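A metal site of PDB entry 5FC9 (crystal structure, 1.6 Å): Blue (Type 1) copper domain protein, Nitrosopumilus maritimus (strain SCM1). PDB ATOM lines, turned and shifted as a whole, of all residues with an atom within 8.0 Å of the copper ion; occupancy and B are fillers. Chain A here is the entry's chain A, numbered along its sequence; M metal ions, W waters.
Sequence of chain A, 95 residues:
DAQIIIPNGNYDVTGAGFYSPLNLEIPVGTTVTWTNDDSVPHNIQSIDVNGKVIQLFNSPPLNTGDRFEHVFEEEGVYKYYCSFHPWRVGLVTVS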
ATOM      1  N   ILE A   6      -7.301  35.096 -29.026  1.00  0.00           N
ATOM      2  CA  ILE A   6      -7.928  33.904 -28.460  1.00  0.00           C
ATOM      3  C   ILE A   6      -6.791  32.980 -28.013  1.00  0.00           C
ATOM      4  O   ILE A   6      -6.074  32.434 -28.840  1.00  0.00           O
ATOM      5  CB  ILE A   6      -8.842  33.178 -29.478  1.00  0.00           C
ATOM      6  CG1 ILE A   6      -9.785  34.168 -30.186  1.00  0.00           C
ATOM      7  CG2 ILE A   6      -9.636  32.090 -28.781  1.00  0.00           C
ATOM      8  CD1 ILE A   6     -10.559  33.525 -31.322  1.00  0.00           C
ATOM      9  N   ASN A  10      -8.472  28.437 -24.507  1.00  0.00           N
ATOM     10  CA  ASN A  10      -9.793  29.069 -24.581  1.00  0.00           C
ATOM     11  C   ASN A  10     -10.927  28.037 -24.684  1.00  0.00           C
ATOM     12  O   ASN A  10     -12.065  28.300 -24.281  1.00  0.00           O
ATOM     13  CB  ASN A  10      -9.811  30.053 -25.775  1.00  0.00           C
ATOM     14  CG  ASN A  10     -11.140  30.789 -25.909  1.00  0.00           C
ATOM     15  OD1 ASN A  10     -11.993  30.394 -26.702  1.00  0.00           O
ATOM     16  ND2 ASN A  10     -11.326  31.851 -25.122  1.00  0.00           N
ATOM     17  N   TYR A  11     -10.627  26.850 -25.194  1.00  0.00           N
ATOM     18  CA  TYR A  11     -11.639  25.786 -25.261  1.00  0.00           C
ATOM     19  C   TYR A  11     -12.045  25.252 -23.881  1.00  0.00           C
ATOM     20  O   TYR A  11     -13.041  24.549 -23.760  1.00  0.00           O
ATOM     21  CB  TYR A  11     -11.148  24.618 -26.120  1.00  0.00           C
ATOM     22  CG  TYR A  11      -9.908  23.944 -25.592  1.00  0.00           C
ATOM     23  CD1 TYR A  11      -8.643  24.348 -26.005  1.00  0.00           C
ATOM     24  CD2 TYR A  11      -9.986  22.911 -24.665  1.00  0.00           C
ATOM     25  CE1 TYR A  11      -7.500  23.739 -25.524  1.00  0.00           C
ATOM     26  CE2 TYR A  11      -8.843  22.294 -24.178  1.00  0.00           C
ATOM     27  CZ  TYR A  11      -7.612  22.722 -24.604  1.00  0.00           C
ATOM     28  OH  TYR A  11      -6.466  22.114 -24.139  1.00  0.00           O
ATOM     29  N   TYR A  19     -10.771  35.585 -23.787  1.00  0.00           N
ATOM     30  CA  TYR A  19     -10.231  36.519 -24.786  1.00  0.00           C
ATOM     31  C   TYR A  19      -9.385  37.596 -24.133  1.00  0.00           C
ATOM     32  O   TYR A  19      -9.711  38.064 -23.048  1.00  0.00           O
ATOM     33  CB  TYR A  19     -11.369  37.176 -25.571  1.00  0.00           C
ATOM     34  CG  TYR A  19     -12.346  36.213 -26.192  1.00  0.00           C
ATOM     35  CD1 TYR A  19     -11.915  35.108 -26.911  1.00  0.00           C
ATOM     36  CD2 TYR A  19     -13.712  36.398 -26.039  1.00  0.00           C
ATOM     37  CE1 TYR A  19     -12.807  34.212 -27.467  1.00  0.00           C
ATOM     38  CE2 TYR A  19     -14.627  35.512 -26.576  1.00  0.00           C
ATOM     39  CZ  TYR A  19     -14.169  34.414 -27.289  1.00  0.00           C
ATOM     40  OH  TYR A  19     -15.051  33.509 -27.843  1.00  0.00           O
ATOM     41  N   ASN A  36      -6.624  33.627 -33.678  1.00  0.00           N
ATOM     42  CA  ASN A  36      -6.774  32.378 -32.947  1.00  0.00           C
ATOM     43  C   ASN A  36      -5.415  31.744 -32.615  1.00  0.00           C
ATOM     44  O   ASN A  36      -4.781  31.157 -33.487  1.00  0.00           O
ATOM     45  CB  ASN A  36      -7.625  31.376 -33.738  1.00  0.00           C
ATOM     46  CG  ASN A  36      -7.914  30.107 -32.937  1.00  0.00           C
ATOM     47  OD1 ASN A  36      -7.636  30.070 -31.742  1.00  0.00           O
ATOM     48  ND2 ASN A  36      -8.441  29.072 -33.589  1.00  0.00           N
ATOM     49  N   ASP A  38      -5.235  29.510 -30.196  1.00  0.00           N
ATOM     50  CA  ASP A  38      -5.600  28.250 -29.566  1.00  0.00           C
ATOM     51  C   ASP A  38      -5.365  27.071 -30.516  1.00  0.00           C
ATOM     52  O   ASP A  38      -5.167  27.247 -31.723  1.00  0.00           O
ATOM     53  CB  ASP A  38      -7.071  28.301 -29.125  1.00  0.00           C
ATOM     54  CG  ASP A  38      -7.384  27.369 -27.970  1.00  0.00           C
ATOM     55  OD1 ASP A  38      -6.477  26.615 -27.532  1.00  0.00           O
ATOM     56  OD2 ASP A  38      -8.541  27.388 -27.511  1.00  0.00           O
ATOM     57  N   VAL A  40      -7.527  24.649 -31.232  1.00  0.00           N
ATOM     58  CA  VAL A  40      -8.772  24.161 -31.820  1.00  0.00           C
ATOM     59  C   VAL A  40      -9.435  25.293 -32.606  1.00  0.00           C
ATOM     60  O   VAL A  40      -9.115  26.457 -32.387  1.00  0.00           O
ATOM     61  CB  VAL A  40      -9.770  23.612 -30.759  1.00  0.00           C
ATOM     62  CG1 VAL A  40      -9.137  22.472 -29.963  1.00  0.00           C
ATOM     63  CG2 VAL A  40     -10.263  24.738 -29.839  1.00  0.00           C
ATOM     64  N   PRO A  41     -10.362  24.966 -33.517  1.00  0.00           N
ATOM     65  CA  PRO A  41     -11.057  26.045 -34.230  1.00  0.00           C
ATOM     66  C   PRO A  41     -11.923  26.900 -33.314  1.00  0.00           C
ATOM     67  O   PRO A  41     -12.468  26.420 -32.310  1.00  0.00           O
ATOM     68  CB  PRO A  41     -11.929  25.301 -35.245  1.00  0.00           C
ATOM     69  CG  PRO A  41     -11.320  23.961 -35.379  1.00  0.00           C
ATOM     70  CD  PRO A  41     -10.737  23.638 -34.036  1.00  0.00           C
ATOM     71  N   HIS A  42     -12.052  28.178 -33.666  1.00  0.00           N
ATOM     72  CA  HIS A  42     -12.931  29.106 -32.979  1.00  0.00           C
ATOM     73  C   HIS A  42     -13.637  29.941 -34.013  1.00  0.00           C
ATOM     74  O   HIS A  42     -13.242  29.962 -35.163  1.00  0.00           O
ATOM     75  CB  HIS A  42     -12.141  30.010 -32.036  1.00  0.00           C
ATOM     76  CG  HIS A  42     -11.632  29.295 -30.824  1.00  0.00           C
ATOM     77  ND1 HIS A  42     -12.459  28.797 -29.847  1.00  0.00           N
ATOM     78  CD2 HIS A  42     -10.371  28.985 -30.445  1.00  0.00           C
ATOM     79  CE1 HIS A  42     -11.737  28.218 -28.905  1.00  0.00           C
ATOM     80  NE2 HIS A  42     -10.457  28.323 -29.240  1.00  0.00           N
ATOM     81  N   ASN A  43     -14.680  30.640 -33.596  1.00  0.00           N
ATOM     82  CA  ASN A  43     -15.212  31.691 -34.454  1.00  0.00           C
ATOM     83  C   ASN A  43     -15.606  32.888 -33.590  1.00  0.00           C
ATOM     84  O   ASN A  43     -15.571  32.830 -32.360  1.00  0.00           O
ATOM     85  CB  ASN A  43     -16.380  31.187 -35.310  1.00  0.00           C
ATOM     86  CG  ASN A  43     -17.539  30.661 -34.491  1.00  0.00           C
ATOM     87  OD1 ASN A  43     -18.089  31.378 -33.657  1.00  0.00           O
ATOM     88  ND2 ASN A  43     -17.920  29.424 -34.715  1.00  0.00           N
ATOM     89  N   ILE A  44     -15.924  33.992 -34.267  1.00  0.00           N
ATOM     90  CA  ILE A  44     -16.290  35.227 -33.601  1.00  0.00           C
ATOM     91  C   ILE A  44     -17.646  35.658 -34.141  1.00  0.00           C
ATOM     92  O   ILE A  44     -17.778  35.938 -35.329  1.00  0.00           O
ATOM     93  CB  ILE A  44     -15.242  36.341 -33.844  1.00  0.00           C
ATOM     94  CG1 ILE A  44     -13.878  35.958 -33.234  1.00  0.00           C
ATOM     95  CG2 ILE A  44     -15.730  37.676 -33.293  1.00  0.00           C
ATOM     96  CD1 ILE A  44     -13.893  35.792 -31.726  1.00  0.00           C
ATOM     97  N   LEU A  62     -12.171  29.915 -37.645  1.00  0.00           N
ATOM     98  CA  LEU A  62     -10.779  30.333 -37.562  1.00  0.00           C
ATOM     99  C   LEU A  62      -9.921  29.157 -37.163  1.00  0.00           C
ATOM    100  O   LEU A  62     -10.018  28.666 -36.026  1.00  0.00           O
ATOM    101  CB  LEU A  62     -10.611  31.467 -36.538  1.00  0.00           C
ATOM    102  CG  LEU A  62     -11.528  32.672 -36.759  1.00  0.00           C
ATOM    103  CD1 LEU A  62     -11.372  33.688 -35.639  1.00  0.00           C
ATOM    104  CD2 LEU A  62     -11.205  33.289 -38.110  1.00  0.00           C
ATOM    105  N   TYR A  81     -19.421  36.195 -29.133  1.00  0.00           N
ATOM    106  CA  TYR A  81     -19.058  34.921 -28.535  1.00  0.00           C
ATOM    107  C   TYR A  81     -18.478  34.021 -29.623  1.00  0.00           C
ATOM    108  O   TYR A  81     -18.251  34.474 -30.751  1.00  0.00           O
ATOM    109  CB  TYR A  81     -20.301  34.344 -27.808  1.00  0.00           C
ATOM    110  CG  TYR A  81     -21.267  33.470 -28.586  1.00  0.00           C
ATOM    111  CD1 TYR A  81     -22.011  32.499 -27.924  1.00  0.00           C
ATOM    112  CD2 TYR A  81     -21.391  33.544 -29.970  1.00  0.00           C
ATOM    113  CE1 TYR A  81     -22.888  31.668 -28.621  1.00  0.00           C
ATOM    114  CE2 TYR A  81     -22.246  32.715 -30.667  1.00  0.00           C
ATOM    115  CZ  TYR A  81     -22.997  31.780 -29.987  1.00  0.00           C
ATOM    116  OH  TYR A  81     -23.866  30.968 -30.675  1.00  0.00           O
ATOM    117  N   CYS A  82     -18.222  32.781 -29.276  1.00  0.00           N
ATOM    118  CA  CYS A  82     -17.847  31.736 -30.217  1.00  0.00           C
ATOM    119  C   CYS A  82     -18.948  30.693 -30.218  1.00  0.00           C
ATOM    120  O   CYS A  82     -19.337  30.219 -29.145  1.00  0.00           O
ATOM    121  CB  CYS A  82     -16.514  31.086 -29.816  1.00  0.00           C
ATOM    122  SG  CYS A  82     -16.073  29.610 -30.759  1.00  0.00           S
ATOM    123  N   SER A  83     -19.453  30.311 -31.378  1.00  0.00           N
ATOM    124  CA  SER A  83     -20.574  29.381 -31.371  1.00  0.00           C
ATOM    125  C   SER A  83     -20.167  27.968 -30.914  1.00  0.00           C
ATOM    126  O   SER A  83     -21.001  27.184 -30.479  1.00  0.00           O
ATOM    127  CB  SER A  83     -21.271  29.340 -32.745  1.00  0.00           C
ATOM    128  OG  SER A  83     -20.458  28.724 -33.728  1.00  0.00           O
ATOM    129  N   PHE A  84     -18.866  27.658 -30.988  1.00  0.00           N
ATOM    130  CA  PHE A  84     -18.379  26.369 -30.506  1.00  0.00           C
ATOM    131  C   PHE A  84     -18.208  26.364 -28.994  1.00  0.00           C
ATOM    132  O   PHE A  84     -18.324  25.321 -28.343  1.00  0.00           O
ATOM    133  CB  PHE A  84     -17.040  26.021 -31.143  1.00  0.00           C
ATOM    134  CG  PHE A  84     -17.024  26.098 -32.638  1.00  0.00           C
ATOM    135  CD1 PHE A  84     -18.129  25.728 -33.384  1.00  0.00           C
ATOM    136  CD2 PHE A  84     -15.889  26.524 -33.298  1.00  0.00           C
ATOM    137  CE1 PHE A  84     -18.108  25.797 -34.766  1.00  0.00           C
ATOM    138  CE2 PHE A  84     -15.854  26.598 -34.677  1.00  0.00           C
ATOM    139  CZ  PHE A  84     -16.964  26.234 -35.411  1.00  0.00           C
ATOM    140  N   HIS A  85     -17.893  27.534 -28.445  1.00  0.00           N
ATOM    141  CA  HIS A  85     -17.693  27.669 -27.001  1.00  0.00           C
ATOM    142  C   HIS A  85     -18.455  28.879 -26.513  1.00  0.00           C
ATOM    143  O   HIS A  85     -17.876  29.909 -26.235  1.00  0.00           O
ATOM    144  CB  HIS A  85     -16.206  27.786 -26.663  1.00  0.00           C
ATOM    145  CG  HIS A  85     -15.355  26.794 -27.384  1.00  0.00           C
ATOM    146  ND1 HIS A  85     -14.646  27.106 -28.523  1.00  0.00           N
ATOM    147  CD2 HIS A  85     -15.114  25.482 -27.140  1.00  0.00           C
ATOM    148  CE1 HIS A  85     -13.999  26.033 -28.951  1.00  0.00           C
ATOM    149  NE2 HIS A  85     -14.279  25.031 -28.137  1.00  0.00           N
ATOM    150  N   PRO A  86     -19.793  28.757 -26.422  1.00  0.00           N
ATOM    151  CA  PRO A  86     -20.635  29.935 -26.195  1.00  0.00           C
ATOM    152  C   PRO A  86     -20.450  30.593 -24.820  1.00  0.00           C
ATOM    153  O   PRO A  86     -20.868  31.738 -24.652  1.00  0.00           O
ATOM    154  CB  PRO A  86     -22.053  29.387 -26.358  1.00  0.00           C
ATOM    155  CG  PRO A  86     -21.941  27.935 -26.169  1.00  0.00           C
ATOM    156  CD  PRO A  86     -20.591  27.547 -26.670  1.00  0.00           C
ATOM    157  N   TRP A  87     -19.819  29.890 -23.883  1.00  0.00           N
ATOM    158  CA  TRP A  87     -19.493  30.496 -22.593  1.00  0.00           C
ATOM    159  C   TRP A  87     -18.372  31.519 -22.713  1.00  0.00           C
ATOM    160  O   TRP A  87     -18.150  32.334 -21.811  1.00  0.00           O
ATOM    161  CB  TRP A  87     -19.108  29.422 -21.562  1.00  0.00           C
ATOM    162  CG  TRP A  87     -17.918  28.605 -21.949  1.00  0.00           C
ATOM    163  CD1 TRP A  87     -16.602  28.813 -21.606  1.00  0.00           C
ATOM    164  CD2 TRP A  87     -17.932  27.417 -22.759  1.00  0.00           C
ATOM    165  NE1 TRP A  87     -15.804  27.843 -22.160  1.00  0.00           N
ATOM    166  CE2 TRP A  87     -16.598  26.981 -22.882  1.00  0.00           C
ATOM    167  CE3 TRP A  87     -18.948  26.698 -23.390  1.00  0.00           C
ATOM    168  CZ2 TRP A  87     -16.262  25.839 -23.601  1.00  0.00           C
ATOM    169  CZ3 TRP A  87     -18.605  25.571 -24.124  1.00  0.00           C
ATOM    170  CH2 TRP A  87     -17.273  25.155 -24.234  1.00  0.00           C
ATOM    171  N   ARG A  88     -17.671  31.510 -23.840  1.00  0.00           N
ATOM    172  CA  ARG A  88     -16.604  32.480 -24.081  1.00  0.00           C
ATOM    173  C   ARG A  88     -17.164  33.705 -24.750  1.00  0.00           C
ATOM    174  O   ARG A  88     -17.305  33.744 -25.986  1.00  0.00           O
ATOM    175  CB  ARG A  88     -15.498  31.861 -24.929  1.00  0.00           C
ATOM    176  CG  ARG A  88     -14.812  30.672 -24.266  1.00  0.00           C
ATOM    177  CD  ARG A  88     -14.259  31.063 -22.906  1.00  0.00           C
ATOM    178  NE  ARG A  88     -13.242  30.129 -22.450  1.00  0.00           N
ATOM    179  CZ  ARG A  88     -12.510  30.326 -21.354  1.00  0.00           C
ATOM    180  NH1 ARG A  88     -12.747  31.390 -20.606  1.00  0.00           N
ATOM    181  NH2 ARG A  88     -11.564  29.465 -21.009  1.00  0.00           N
HETATM  182 CU    CU M   1     -14.403  28.914 -29.469  1.00  0.00          CU
HETATM  183  O   HOH W   1     -14.168  30.594 -27.998  1.00  0.00           O
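The side-chain sulfur (SG) of Cys 82 lies close to the backbone NH (N) of Asn 43 (3.3 Å). The side-chain sulfur (SG) of Cys 82 sits close to the backbone NH (N) of Phe 84 (3.4 Å). The side-chain carboxylate (OD2) of Asp 38 sits at hydrogen-bond distance from a ring nitrogen (NE2) of His 42. The side-chain carboxylate of Asp 38 sits at hydrogen-bond distance from the backbone NH of Asn 10. O of Asn 10 sits at hydrogen-bond distance from NE of Arg 88 (2.8 Å). O of His 42 sits at hydrogen-bond distance from N of Leu 62 (2.7 Å).
Asn 10 touches the copper ion (OD1 to CU, 3.96 Å). Within 4 Å of the copper ion: Asn 10, His 42, Cys 82 and His 85.
The copper ion is bound by a ring nitrogen (ND1) of His 42, a ring nitrogen (ND1) of His 85, the side-chain sulfur (SG) of Cys 82 and water W1. The copper ion has four donor atoms within binding distance.
Water W1 bridges the side-chain amide oxygen (OD1) of Asn 10 (2.5 Å) and the side-chain hydroxyl (OH) of Tyr 19 (3.0 Å).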
